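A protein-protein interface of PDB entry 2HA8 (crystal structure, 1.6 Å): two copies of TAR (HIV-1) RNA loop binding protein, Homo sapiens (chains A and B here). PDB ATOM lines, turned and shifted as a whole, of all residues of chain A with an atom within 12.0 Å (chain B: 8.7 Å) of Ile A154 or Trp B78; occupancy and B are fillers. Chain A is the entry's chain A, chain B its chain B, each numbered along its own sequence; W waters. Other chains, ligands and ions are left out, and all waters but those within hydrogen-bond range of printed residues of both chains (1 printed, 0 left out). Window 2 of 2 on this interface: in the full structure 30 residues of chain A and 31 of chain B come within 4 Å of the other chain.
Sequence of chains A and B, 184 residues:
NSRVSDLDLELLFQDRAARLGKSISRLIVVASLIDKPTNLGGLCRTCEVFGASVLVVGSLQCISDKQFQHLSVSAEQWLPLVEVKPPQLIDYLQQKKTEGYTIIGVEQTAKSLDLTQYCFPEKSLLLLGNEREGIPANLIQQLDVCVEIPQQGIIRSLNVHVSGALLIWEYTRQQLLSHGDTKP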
ATOM      1  N   GLN A 108       2.997 -18.738  -5.721  1.00  0.00           N
ATOM      2  CA  GLN A 108       3.319 -19.588  -4.572  1.00  0.00           C
ATOM      3  C   GLN A 108       1.990 -19.957  -3.906  1.00  0.00           C
ATOM      4  O   GLN A 108       1.297 -19.074  -3.402  1.00  0.00           O
ATOM      5  CB  GLN A 108       4.225 -18.834  -3.586  1.00  0.00           C
ATOM      6  CG  GLN A 108       5.544 -18.353  -4.203  1.00  0.00           C
ATOM      7  CD  GLN A 108       6.310 -17.429  -3.274  1.00  0.00           C
ATOM      8  OE1 GLN A 108       5.949 -16.268  -3.090  1.00  0.00           O
ATOM      9  NE2 GLN A 108       7.364 -17.947  -2.689  1.00  0.00           N
ATOM     10  N   ILE A 149       8.362 -21.028  -8.145  1.00  0.00           N
ATOM     11  CA  ILE A 149       9.824 -21.075  -8.120  1.00  0.00           C
ATOM     12  C   ILE A 149      10.233 -21.364  -6.682  1.00  0.00           C
ATOM     13  O   ILE A 149       9.856 -20.616  -5.798  1.00  0.00           O
ATOM     14  CB  ILE A 149      10.383 -19.708  -8.528  1.00  0.00           C
ATOM     15  CG1 ILE A 149       9.896 -19.332  -9.947  1.00  0.00           C
ATOM     16  CG2 ILE A 149      11.897 -19.708  -8.475  1.00  0.00           C
ATOM     17  CD1 ILE A 149       9.875 -17.839 -10.227  1.00  0.00           C
ATOM     18  N   PRO A 150      11.009 -22.442  -6.448  1.00  0.00           N
ATOM     19  CA  PRO A 150      11.412 -22.745  -5.047  1.00  0.00           C
ATOM     20  C   PRO A 150      12.381 -21.687  -4.501  1.00  0.00           C
ATOM     21  O   PRO A 150      13.252 -21.215  -5.235  1.00  0.00           O
ATOM     22  CB  PRO A 150      12.115 -24.103  -5.159  1.00  0.00           C
ATOM     23  CG  PRO A 150      12.605 -24.155  -6.589  1.00  0.00           C
ATOM     24  CD  PRO A 150      11.547 -23.421  -7.409  1.00  0.00           C
ATOM     25  N   GLN A 151      12.234 -21.334  -3.228  1.00  0.00           N
ATOM     26  CA  GLN A 151      13.073 -20.309  -2.595  1.00  0.00           C
ATOM     27  C   GLN A 151      13.831 -20.907  -1.406  1.00  0.00           C
ATOM     28  O   GLN A 151      13.403 -21.913  -0.835  1.00  0.00           O
ATOM     29  CB  GLN A 151      12.225 -19.122  -2.138  1.00  0.00           C
ATOM     30  CG  GLN A 151      11.463 -18.427  -3.262  1.00  0.00           C
ATOM     31  CD  GLN A 151      10.781 -17.165  -2.823  1.00  0.00           C
ATOM     32  OE1 GLN A 151      10.849 -16.757  -1.643  1.00  0.00           O
ATOM     33  NE2 GLN A 151      10.129 -16.520  -3.747  1.00  0.00           N
ATOM     34  N   GLN A 152      14.958 -20.293  -1.049  1.00  0.00           N
ATOM     35  CA  GLN A 152      15.783 -20.798   0.053  1.00  0.00           C
ATOM     36  C   GLN A 152      15.934 -19.801   1.193  1.00  0.00           C
ATOM     37  O   GLN A 152      16.140 -20.196   2.352  1.00  0.00           O
ATOM     38  CB  GLN A 152      17.168 -21.130  -0.452  1.00  0.00           C
ATOM     39  CG  GLN A 152      17.219 -22.146  -1.542  1.00  0.00           C
ATOM     40  CD  GLN A 152      18.607 -22.273  -2.100  1.00  0.00           C
ATOM     41  OE1 GLN A 152      19.605 -22.135  -1.375  1.00  0.00           O
ATOM     42  NE2 GLN A 152      18.692 -22.539  -3.393  1.00  0.00           N
ATOM     43  N   GLY A 153      15.846 -18.515   0.881  1.00  0.00           N
ATOM     44  CA  GLY A 153      16.109 -17.484   1.873  1.00  0.00           C
ATOM     45  C   GLY A 153      14.922 -17.104   2.744  1.00  0.00           C
ATOM     46  O   GLY A 153      13.925 -17.841   2.850  1.00  0.00           O
ATOM     47  N   ILE A 154      15.028 -15.920   3.344  1.00  0.00           N
ATOM     48  CA  ILE A 154      14.036 -15.382   4.263  1.00  0.00           C
ATOM     49  C   ILE A 154      12.957 -14.528   3.586  1.00  0.00           C
ATOM     50  O   ILE A 154      11.798 -14.516   4.015  1.00  0.00           O
ATOM     51  CB  ILE A 154      14.738 -14.523   5.368  1.00  0.00           C
ATOM     52  CG1 ILE A 154      15.784 -15.348   6.127  1.00  0.00           C
ATOM     53  CG2 ILE A 154      13.727 -13.879   6.293  1.00  0.00           C
ATOM     54  CD1 ILE A 154      15.313 -16.691   6.670  1.00  0.00           C
ATOM     55  N   ILE A 155      13.346 -13.801   2.536  1.00  0.00           N
ATOM     56  CA  ILE A 155      12.428 -12.922   1.831  1.00  0.00           C
ATOM     57  C   ILE A 155      11.298 -13.766   1.203  1.00  0.00           C
ATOM     58  O   ILE A 155      11.539 -14.844   0.655  1.00  0.00           O
ATOM     59  CB  ILE A 155      13.162 -12.054   0.769  1.00  0.00           C
ATOM     60  CG1 ILE A 155      14.160 -11.099   1.440  1.00  0.00           C
ATOM     61  CG2 ILE A 155      12.172 -11.280  -0.096  1.00  0.00           C
ATOM     62  CD1 ILE A 155      13.582 -10.201   2.498  1.00  0.00           C
ATOM     63  N   ARG A 156      10.075 -13.270   1.302  1.00  0.00           N
ATOM     64  CA  ARG A 156       8.903 -14.102   0.996  1.00  0.00           C
ATOM     65  C   ARG A 156       8.688 -14.416  -0.477  1.00  0.00           C
ATOM     66  O   ARG A 156       8.099 -15.444  -0.801  1.00  0.00           O
ATOM     67  CB  ARG A 156       7.623 -13.488   1.583  1.00  0.00           C
ATOM     68  CG  ARG A 156       7.277 -12.077   1.140  1.00  0.00           C
ATOM     69  CD  ARG A 156       6.243 -11.449   2.100  1.00  0.00           C
ATOM     70  NE  ARG A 156       5.126 -12.367   2.346  1.00  0.00           N
ATOM     71  CZ  ARG A 156       4.400 -12.407   3.463  1.00  0.00           C
ATOM     72  NH1 ARG A 156       4.643 -11.561   4.462  1.00  0.00           N
ATOM     73  NH2 ARG A 156       3.419 -13.295   3.578  1.00  0.00           N
ATOM     74  N   SER A 157       9.140 -13.529  -1.353  1.00  0.00           N
ATOM     75  CA  SER A 157       8.812 -13.650  -2.790  1.00  0.00           C
ATOM     76  C   SER A 157       9.863 -12.964  -3.648  1.00  0.00           C
ATOM     77  O   SER A 157      10.605 -12.121  -3.163  1.00  0.00           O
ATOM     78  CB  SER A 157       7.454 -13.018  -3.059  1.00  0.00           C
ATOM     79  OG  SER A 157       7.476 -11.621  -2.793  1.00  0.00           O
ATOM     80  N   LEU A 158       9.907 -13.333  -4.926  1.00  0.00           N
ATOM     81  CA  LEU A 158      10.674 -12.610  -5.922  1.00  0.00           C
ATOM     82  C   LEU A 158       9.878 -11.422  -6.469  1.00  0.00           C
ATOM     83  O   LEU A 158       8.659 -11.354  -6.306  1.00  0.00           O
ATOM     84  CB  LEU A 158      11.030 -13.559  -7.067  1.00  0.00           C
ATOM     85  CG  LEU A 158      12.009 -14.688  -6.718  1.00  0.00           C
ATOM     86  CD1 LEU A 158      11.861 -15.809  -7.752  1.00  0.00           C
ATOM     87  CD2 LEU A 158      13.458 -14.145  -6.736  1.00  0.00           C
ATOM     88  N   ASN A 159      10.569 -10.492  -7.112  1.00  0.00           N
ATOM     89  CA  ASN A 159       9.915  -9.482  -7.908  1.00  0.00           C
ATOM     90  C   ASN A 159       9.131 -10.166  -9.046  1.00  0.00           C
ATOM     91  O   ASN A 159       9.550 -11.230  -9.567  1.00  0.00           O
ATOM     92  CB  ASN A 159      10.960  -8.512  -8.464  1.00  0.00           C
ATOM     93  CG  ASN A 159      10.425  -7.646  -9.570  1.00  0.00           C
ATOM     94  OD1 ASN A 159      10.502  -8.016 -10.749  1.00  0.00           O
ATOM     95  ND2 ASN A 159       9.904  -6.474  -9.214  1.00  0.00           N
ATOM     96  N   CYS B  44      20.087  -7.829  -5.123  1.00  0.00           N
ATOM     97  CA  CYS B  44      20.176  -8.198  -3.718  1.00  0.00           C
ATOM     98  C   CYS B  44      18.997  -9.089  -3.324  1.00  0.00           C
ATOM     99  O   CYS B  44      19.191 -10.138  -2.696  1.00  0.00           O
ATOM    100  CB  CYS B  44      20.229  -6.940  -2.868  1.00  0.00           C
ATOM    101  SG  CYS B  44      20.448  -7.227  -1.109  1.00  0.00           S
ATOM    102  N   ARG B  45      17.788  -8.698  -3.729  1.00  0.00           N
ATOM    103  CA  ARG B  45      16.608  -9.501  -3.396  1.00  0.00           C
ATOM    104  C   ARG B  45      16.712 -10.905  -4.018  1.00  0.00           C
ATOM    105  O   ARG B  45      16.492 -11.916  -3.361  1.00  0.00           O
ATOM    106  CB  ARG B  45      15.351  -8.768  -3.850  1.00  0.00           C
ATOM    107  CG  ARG B  45      14.045  -9.535  -3.604  1.00  0.00           C
ATOM    108  CD  ARG B  45      12.883  -8.799  -4.245  1.00  0.00           C
ATOM    109  NE  ARG B  45      11.605  -9.365  -3.820  1.00  0.00           N
ATOM    110  CZ  ARG B  45      10.431  -8.768  -3.998  1.00  0.00           C
ATOM    111  NH1 ARG B  45      10.349  -7.590  -4.626  1.00  0.00           N
ATOM    112  NH2 ARG B  45       9.325  -9.375  -3.571  1.00  0.00           N
ATOM    113  N   CYS B  47      19.400 -12.610  -5.048  1.00  0.00           N
ATOM    114  CA  CYS B  47      20.460 -13.393  -4.416  1.00  0.00           C
ATOM    115  C   CYS B  47      20.030 -13.971  -3.072  1.00  0.00           C
ATOM    116  O   CYS B  47      20.348 -15.111  -2.766  1.00  0.00           O
ATOM    117  CB  CYS B  47      21.691 -12.518  -4.187  1.00  0.00           C
ATOM    118  SG  CYS B  47      22.602 -12.201  -5.693  1.00  0.00           S
ATOM    119  N   GLU B  48      19.321 -13.169  -2.283  1.00  0.00           N
ATOM    120  CA  GLU B  48      18.849 -13.616  -0.975  1.00  0.00           C
ATOM    121  C   GLU B  48      17.846 -14.768  -1.096  1.00  0.00           C
ATOM    122  O   GLU B  48      17.978 -15.799  -0.412  1.00  0.00           O
ATOM    123  CB  GLU B  48      18.240 -12.451  -0.197  1.00  0.00           C
ATOM    124  CG  GLU B  48      18.133 -12.728   1.336  1.00  0.00           C
ATOM    125  CD  GLU B  48      17.027 -13.714   1.727  1.00  0.00           C
ATOM    126  OE1 GLU B  48      15.977 -13.783   1.050  1.00  0.00           O
ATOM    127  OE2 GLU B  48      17.206 -14.438   2.735  1.00  0.00           O
ATOM    128  N   VAL B  49      16.891 -14.613  -2.019  1.00  0.00           N
ATOM    129  CA  VAL B  49      15.857 -15.616  -2.243  1.00  0.00           C
ATOM    130  C   VAL B  49      16.468 -16.951  -2.650  1.00  0.00           C
ATOM    131  O   VAL B  49      16.005 -18.028  -2.225  1.00  0.00           O
ATOM    132  CB  VAL B  49      14.853 -15.118  -3.311  1.00  0.00           C
ATOM    133  CG1 VAL B  49      14.004 -16.270  -3.812  1.00  0.00           C
ATOM    134  CG2 VAL B  49      13.993 -13.936  -2.759  1.00  0.00           C
ATOM    135  N   PHE B  50      17.522 -16.902  -3.472  1.00  0.00           N
ATOM    136  CA  PHE B  50      18.171 -18.137  -3.932  1.00  0.00           C
ATOM    137  C   PHE B  50      19.348 -18.619  -3.086  1.00  0.00           C
ATOM    138  O   PHE B  50      20.022 -19.592  -3.435  1.00  0.00           O
ATOM    139  CB  PHE B  50      18.566 -18.020  -5.420  1.00  0.00           C
ATOM    140  CG  PHE B  50      17.387 -18.033  -6.333  1.00  0.00           C
ATOM    141  CD1 PHE B  50      16.492 -19.117  -6.306  1.00  0.00           C
ATOM    142  CD2 PHE B  50      17.115 -16.957  -7.153  1.00  0.00           C
ATOM    143  CE1 PHE B  50      15.366 -19.127  -7.143  1.00  0.00           C
ATOM    144  CE2 PHE B  50      16.012 -16.968  -7.997  1.00  0.00           C
ATOM    145  CZ  PHE B  50      15.129 -18.045  -7.974  1.00  0.00           C
ATOM    146  N   GLY B  51      19.580 -17.961  -1.959  1.00  0.00           N
ATOM    147  CA  GLY B  51      20.619 -18.415  -1.042  1.00  0.00           C
ATOM    148  C   GLY B  51      22.037 -18.302  -1.575  1.00  0.00           C
ATOM    149  O   GLY B  51      22.881 -19.173  -1.294  1.00  0.00           O
ATOM    150  N   ALA B  52      22.322 -17.244  -2.338  1.00  0.00           N
ATOM    151  CA  ALA B  52      23.705 -16.988  -2.770  1.00  0.00           C
ATOM    152  C   ALA B  52      24.588 -16.850  -1.528  1.00  0.00           C
ATOM    153  O   ALA B  52      24.126 -16.358  -0.488  1.00  0.00           O
ATOM    154  CB  ALA B  52      23.778 -15.724  -3.588  1.00  0.00           C
ATOM    155  N   SER B  53      25.841 -17.296  -1.639  1.00  0.00           N
ATOM    156  CA  SER B  53      26.794 -17.225  -0.512  1.00  0.00           C
ATOM    157  C   SER B  53      27.137 -15.789  -0.149  1.00  0.00           C
ATOM    158  O   SER B  53      27.252 -15.433   1.044  1.00  0.00           O
ATOM    159  CB  SER B  53      28.060 -18.007  -0.852  1.00  0.00           C
ATOM    160  OG  SER B  53      27.730 -19.344  -1.257  1.00  0.00           O
ATOM    161  N   VAL B  54      27.315 -14.967  -1.177  1.00  0.00           N
ATOM    162  CA  VAL B  54      27.629 -13.556  -1.002  1.00  0.00           C
ATOM    163  C   VAL B  54      27.289 -12.779  -2.267  1.00  0.00           C
ATOM    164  O   VAL B  54      27.370 -13.314  -3.371  1.00  0.00           O
ATOM    165  CB  VAL B  54      29.118 -13.347  -0.589  1.00  0.00           C
ATOM    166  CG1 VAL B  54      30.040 -13.849  -1.639  1.00  0.00           C
ATOM    167  CG2 VAL B  54      29.422 -11.874  -0.278  1.00  0.00           C
ATOM    168  N   SER B  72      15.320  -3.853  -2.845  1.00  0.00           N
ATOM    169  CA  SER B  72      15.904  -4.974  -2.113  1.00  0.00           C
ATOM    170  C   SER B  72      14.969  -5.532  -1.036  1.00  0.00           C
ATOM    171  O   SER B  72      15.192  -6.634  -0.548  1.00  0.00           O
ATOM    172  CB  SER B  72      17.241  -4.574  -1.488  1.00  0.00           C
ATOM    173  OG  SER B  72      17.033  -3.598  -0.466  1.00  0.00           O
ATOM    174  N   VAL B  73      13.950  -4.745  -0.666  1.00  0.00           N
ATOM    175  CA  VAL B  73      12.931  -5.112   0.337  1.00  0.00           C
ATOM    176  C   VAL B  73      13.493  -5.864   1.565  1.00  0.00           C
ATOM    177  O   VAL B  73      13.005  -6.937   1.966  1.00  0.00           O
ATOM    178  CB  VAL B  73      11.681  -5.806  -0.308  1.00  0.00           C
ATOM    179  CG1 VAL B  73      11.002  -4.861  -1.289  1.00  0.00           C
ATOM    180  CG2 VAL B  73      12.052  -7.133  -0.984  1.00  0.00           C
ATOM    181  N   SER B  74      14.530  -5.265   2.160  1.00  0.00           N
ATOM    182  CA  SER B  74      15.186  -5.782   3.383  1.00  0.00           C
ATOM    183  C   SER B  74      16.086  -6.983   3.187  1.00  0.00           C
ATOM    184  O   SER B  74      16.642  -7.500   4.151  1.00  0.00           O
ATOM    185  CB  SER B  74      14.182  -6.057   4.518  1.00  0.00           C
ATOM    186  OG  SER B  74      13.524  -4.863   4.878  1.00  0.00           O
ATOM    187  N   ALA B  75      16.264  -7.423   1.937  1.00  0.00           N
ATOM    188  CA  ALA B  75      17.110  -8.590   1.684  1.00  0.00           C
ATOM    189  C   ALA B  75      18.533  -8.412   2.237  1.00  0.00           C
ATOM    190  O   ALA B  75      19.202  -9.394   2.600  1.00  0.00           O
ATOM    191  CB  ALA B  75      17.149  -8.903   0.167  1.00  0.00           C
ATOM    192  N   GLU B  76      18.973  -7.158   2.301  1.00  0.00           N
ATOM    193  CA  GLU B  76      20.328  -6.812   2.755  1.00  0.00           C
ATOM    194  C   GLU B  76      20.546  -7.175   4.227  1.00  0.00           C
ATOM    195  O   GLU B  76      21.694  -7.283   4.677  1.00  0.00           O
ATOM    196  CB  GLU B  76      20.635  -5.333   2.505  1.00  0.00           C
ATOM    197  CG  GLU B  76      19.778  -4.315   3.291  1.00  0.00           C
ATOM    198  CD  GLU B  76      18.510  -3.841   2.561  1.00  0.00           C
ATOM    199  OE1 GLU B  76      17.892  -4.601   1.783  1.00  0.00           O
ATOM    200  OE2 GLU B  76      18.097  -2.685   2.783  1.00  0.00           O
ATOM    201  N   GLN B  77      19.450  -7.376   4.958  1.00  0.00           N
ATOM    202  CA  GLN B  77      19.543  -7.825   6.349  1.00  0.00           C
ATOM    203  C   GLN B  77      19.953  -9.280   6.482  1.00  0.00           C
ATOM    204  O   GLN B  77      20.409  -9.714   7.538  1.00  0.00           O
ATOM    205  CB  GLN B  77      18.211  -7.623   7.083  1.00  0.00           C
ATOM    206  CG  GLN B  77      17.859  -6.175   7.331  1.00  0.00           C
ATOM    207  CD  GLN B  77      18.963  -5.420   8.070  1.00  0.00           C
ATOM    208  OE1 GLN B  77      19.585  -5.938   9.011  1.00  0.00           O
ATOM    209  NE2 GLN B  77      19.224  -4.197   7.627  1.00  0.00           N
ATOM    210  N   TRP B  78      19.780 -10.037   5.404  1.00  0.00           N
ATOM    211  CA  TRP B  78      19.833 -11.483   5.462  1.00  0.00           C
ATOM    212  C   TRP B  78      20.848 -12.103   4.511  1.00  0.00           C
ATOM    213  O   TRP B  78      21.081 -13.316   4.562  1.00  0.00           O
ATOM    214  CB  TRP B  78      18.437 -12.046   5.157  1.00  0.00           C
ATOM    215  CG  TRP B  78      17.352 -11.436   6.013  1.00  0.00           C
ATOM    216  CD1 TRP B  78      16.485 -10.447   5.653  1.00  0.00           C
ATOM    217  CD2 TRP B  78      17.048 -11.763   7.371  1.00  0.00           C
ATOM    218  NE1 TRP B  78      15.646 -10.141   6.704  1.00  0.00           N
ATOM    219  CE2 TRP B  78      15.974 -10.933   7.770  1.00  0.00           C
ATOM    220  CE3 TRP B  78      17.578 -12.676   8.288  1.00  0.00           C
ATOM    221  CZ2 TRP B  78      15.409 -11.000   9.051  1.00  0.00           C
ATOM    222  CZ3 TRP B  78      17.012 -12.743   9.567  1.00  0.00           C
ATOM    223  CH2 TRP B  78      15.944 -11.911   9.925  1.00  0.00           C
ATOM    224  N   LEU B  79      21.400 -11.273   3.619  1.00  0.00           N
ATOM    225  CA  LEU B  79      22.352 -11.700   2.601  1.00  0.00           C
ATOM    226  C   LEU B  79      23.725 -11.150   2.960  1.00  0.00           C
ATOM    227  O   LEU B  79      23.848  -9.945   3.176  1.00  0.00           O
ATOM    228  CB  LEU B  79      21.938 -11.130   1.236  1.00  0.00           C
ATOM    229  CG  LEU B  79      22.806 -11.475   0.016  1.00  0.00           C
ATOM    230  CD1 LEU B  79      22.709 -12.958  -0.290  1.00  0.00           C
ATOM    231  CD2 LEU B  79      22.405 -10.635  -1.169  1.00  0.00           C
ATOM    232  N   PRO B  80      24.756 -12.008   3.001  1.00  0.00           N
ATOM    233  CA  PRO B  80      26.127 -11.488   3.159  1.00  0.00           C
ATOM    234  C   PRO B  80      26.529 -10.573   2.005  1.00  0.00           C
ATOM    235  O   PRO B  80      26.362 -10.925   0.829  1.00  0.00           O
ATOM    236  CB  PRO B  80      26.989 -12.753   3.199  1.00  0.00           C
ATOM    237  CG  PRO B  80      26.045 -13.829   3.621  1.00  0.00           C
ATOM    238  CD  PRO B  80      24.745 -13.477   2.956  1.00  0.00           C
ATOM    239  N   LEU B  81      27.008  -9.383   2.348  1.00  0.00           N
ATOM    240  CA  LEU B  81      27.403  -8.403   1.364  1.00  0.00           C
ATOM    241  C   LEU B  81      28.854  -8.012   1.620  1.00  0.00           C
ATOM    242  O   LEU B  81      29.269  -7.863   2.776  1.00  0.00           O
ATOM    243  CB  LEU B  81      26.480  -7.186   1.414  1.00  0.00           C
ATOM    244  CG  LEU B  81      25.076  -7.456   0.827  1.00  0.00           C
ATOM    245  CD1 LEU B  81      24.020  -6.699   1.583  1.00  0.00           C
ATOM    246  CD2 LEU B  81      25.022  -7.115  -0.654  1.00  0.00           C
HETATM  247  O   HOH W   1       6.943  -9.148  -5.200  1.00  0.00           O
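No position is printed for both chains. Of the 19 pairs that touch across the chains among the printed residues, none has its exchanged pair printed and touching as well.
Hydrophobic or aromatic side chains of chain B within 4 Å of the printed part of chain A: Val B49, Phe B50, Ala B75 and Trp B78. Hydrophobic or aromatic side chains of chain A that line the printed part of chain B: Ile A149, Ile A154, Ile A155 and Leu A158. Among the printed residues, 19 pairs touch across the chains. Among the printed residues, no Asp or Glu carboxylate lies within 4 Å of a Lys or Arg side-chain nitrogen of the other chain.
Pro A150 touches Phe B50 (O to CE1, 3.5 Å). Val B49 touches Gln A151. OE1 of Gln A152 touches CA of Gly B51, at 3.9 Å. Gly A153 touches Glu B48. Ile A154 touches Trp B78. Ile A155 touches Val B73. Ala B75 touches Ile A155. CG2 of Val B49 touches O of Ser A157, at 3.9 Å. CD2 of Leu A158 touches CG1 of Val B49, at 3.7 Å. Asn A159 touches Arg B45.
Water W1 lies within hydrogen-bond range of the guanidinium group of Arg B45 (2.9 Å), the backbone carbonyl oxygen of Leu A158 (3.0 Å) and the side-chain hydroxyl of Ser A157 (3.5 Å).
Ile A154 touches just these residues of chain B: Glu B48 (2.7 Å) and Trp B78 (3.9 Å). Of chain A, only Ile A154 (3.9 Å) comes within 4 Å of Trp B78. Of the printed residues of chain B, Gly A153 touches Glu B48 (3.4 Å) and Val B49 (3.1 Å). Glu B48 touches just these residues of chain A: Gly A153 (3.4 Å), Ile A154 (2.7 Å) and Ile A155 (3.0 Å). Val B49 touches just these residues of chain A: Gln A151 (3.4 Å), Gln A152 (2.8 Å), Gly A153 (3.1 Å), Ser A157 (3.9 Å) and Leu A158 (3.7 Å). Ala B75 touches one residue of chain A. No residue of chain A comes within 4 Å of Pro B80. Printed residues of chain A within 4 Å of Arg B45: Ser A157, Leu A158 and Asn A159. Of the printed residues of chain B, Ile A155 touches Glu B48, Val B73 and Ala B75. Printed residues of chain B within 4 Å of Leu A158: Arg B45, Val B49 and Phe B50. Of the printed residues of chain A, Gly B51 touches Gln A152. Ser B53 touches none of the printed residues of chain A. The nearest residue of chain B that does not touch Ile A154 is Val B49 (5.7 Å). The nearest residue of chain A that does not touch Trp B78 is Ile A155 (4.3 Å). The nearest printed residue of chain B that does not touch Ser A157 is Val B73 (5.6 Å).
The side-chain amide nitrogen of Gln A108 lies close to the side-chain amide nitrogen of Gln A151. The backbone carbonyl oxygen of Ile A155 lies close to the side-chain amide oxygen of Gln A151. The backbone NH (N) of Leu A158 lies close to the side-chain amide nitrogen (NE2) of Gln A151 (3.4 Å). O of Arg A156 sits close to OE1 of Gln A151 (3.2 Å).
The backbone carbonyl oxygen of Val B49 lies within hydrogen-bond range of the backbone NH of Gly A153. N of Ile A154 lies within hydrogen-bond range of OE2 of Glu B48, at 2.7 Å. The backbone carbonyl oxygen (O) of Phe B50 is in hydrogen-bond range of the side-chain amide nitrogen (NE2) of Gln A152. The backbone NH of Ile A155 sits at hydrogen-bond distance from the side-chain carboxylate of Glu B48 (3.0 Å). The guanidinium group (NE) of Arg B45 lies within hydrogen-bond range of the backbone carbonyl oxygen (O) of Ser A157. The backbone carbonyl oxygen (O) of Leu A158 is in hydrogen-bond range of the guanidinium group (NH2) of Arg B45, at 3.4 Å. N of Gln A152 lies within hydrogen-bond range of O of Val B49.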
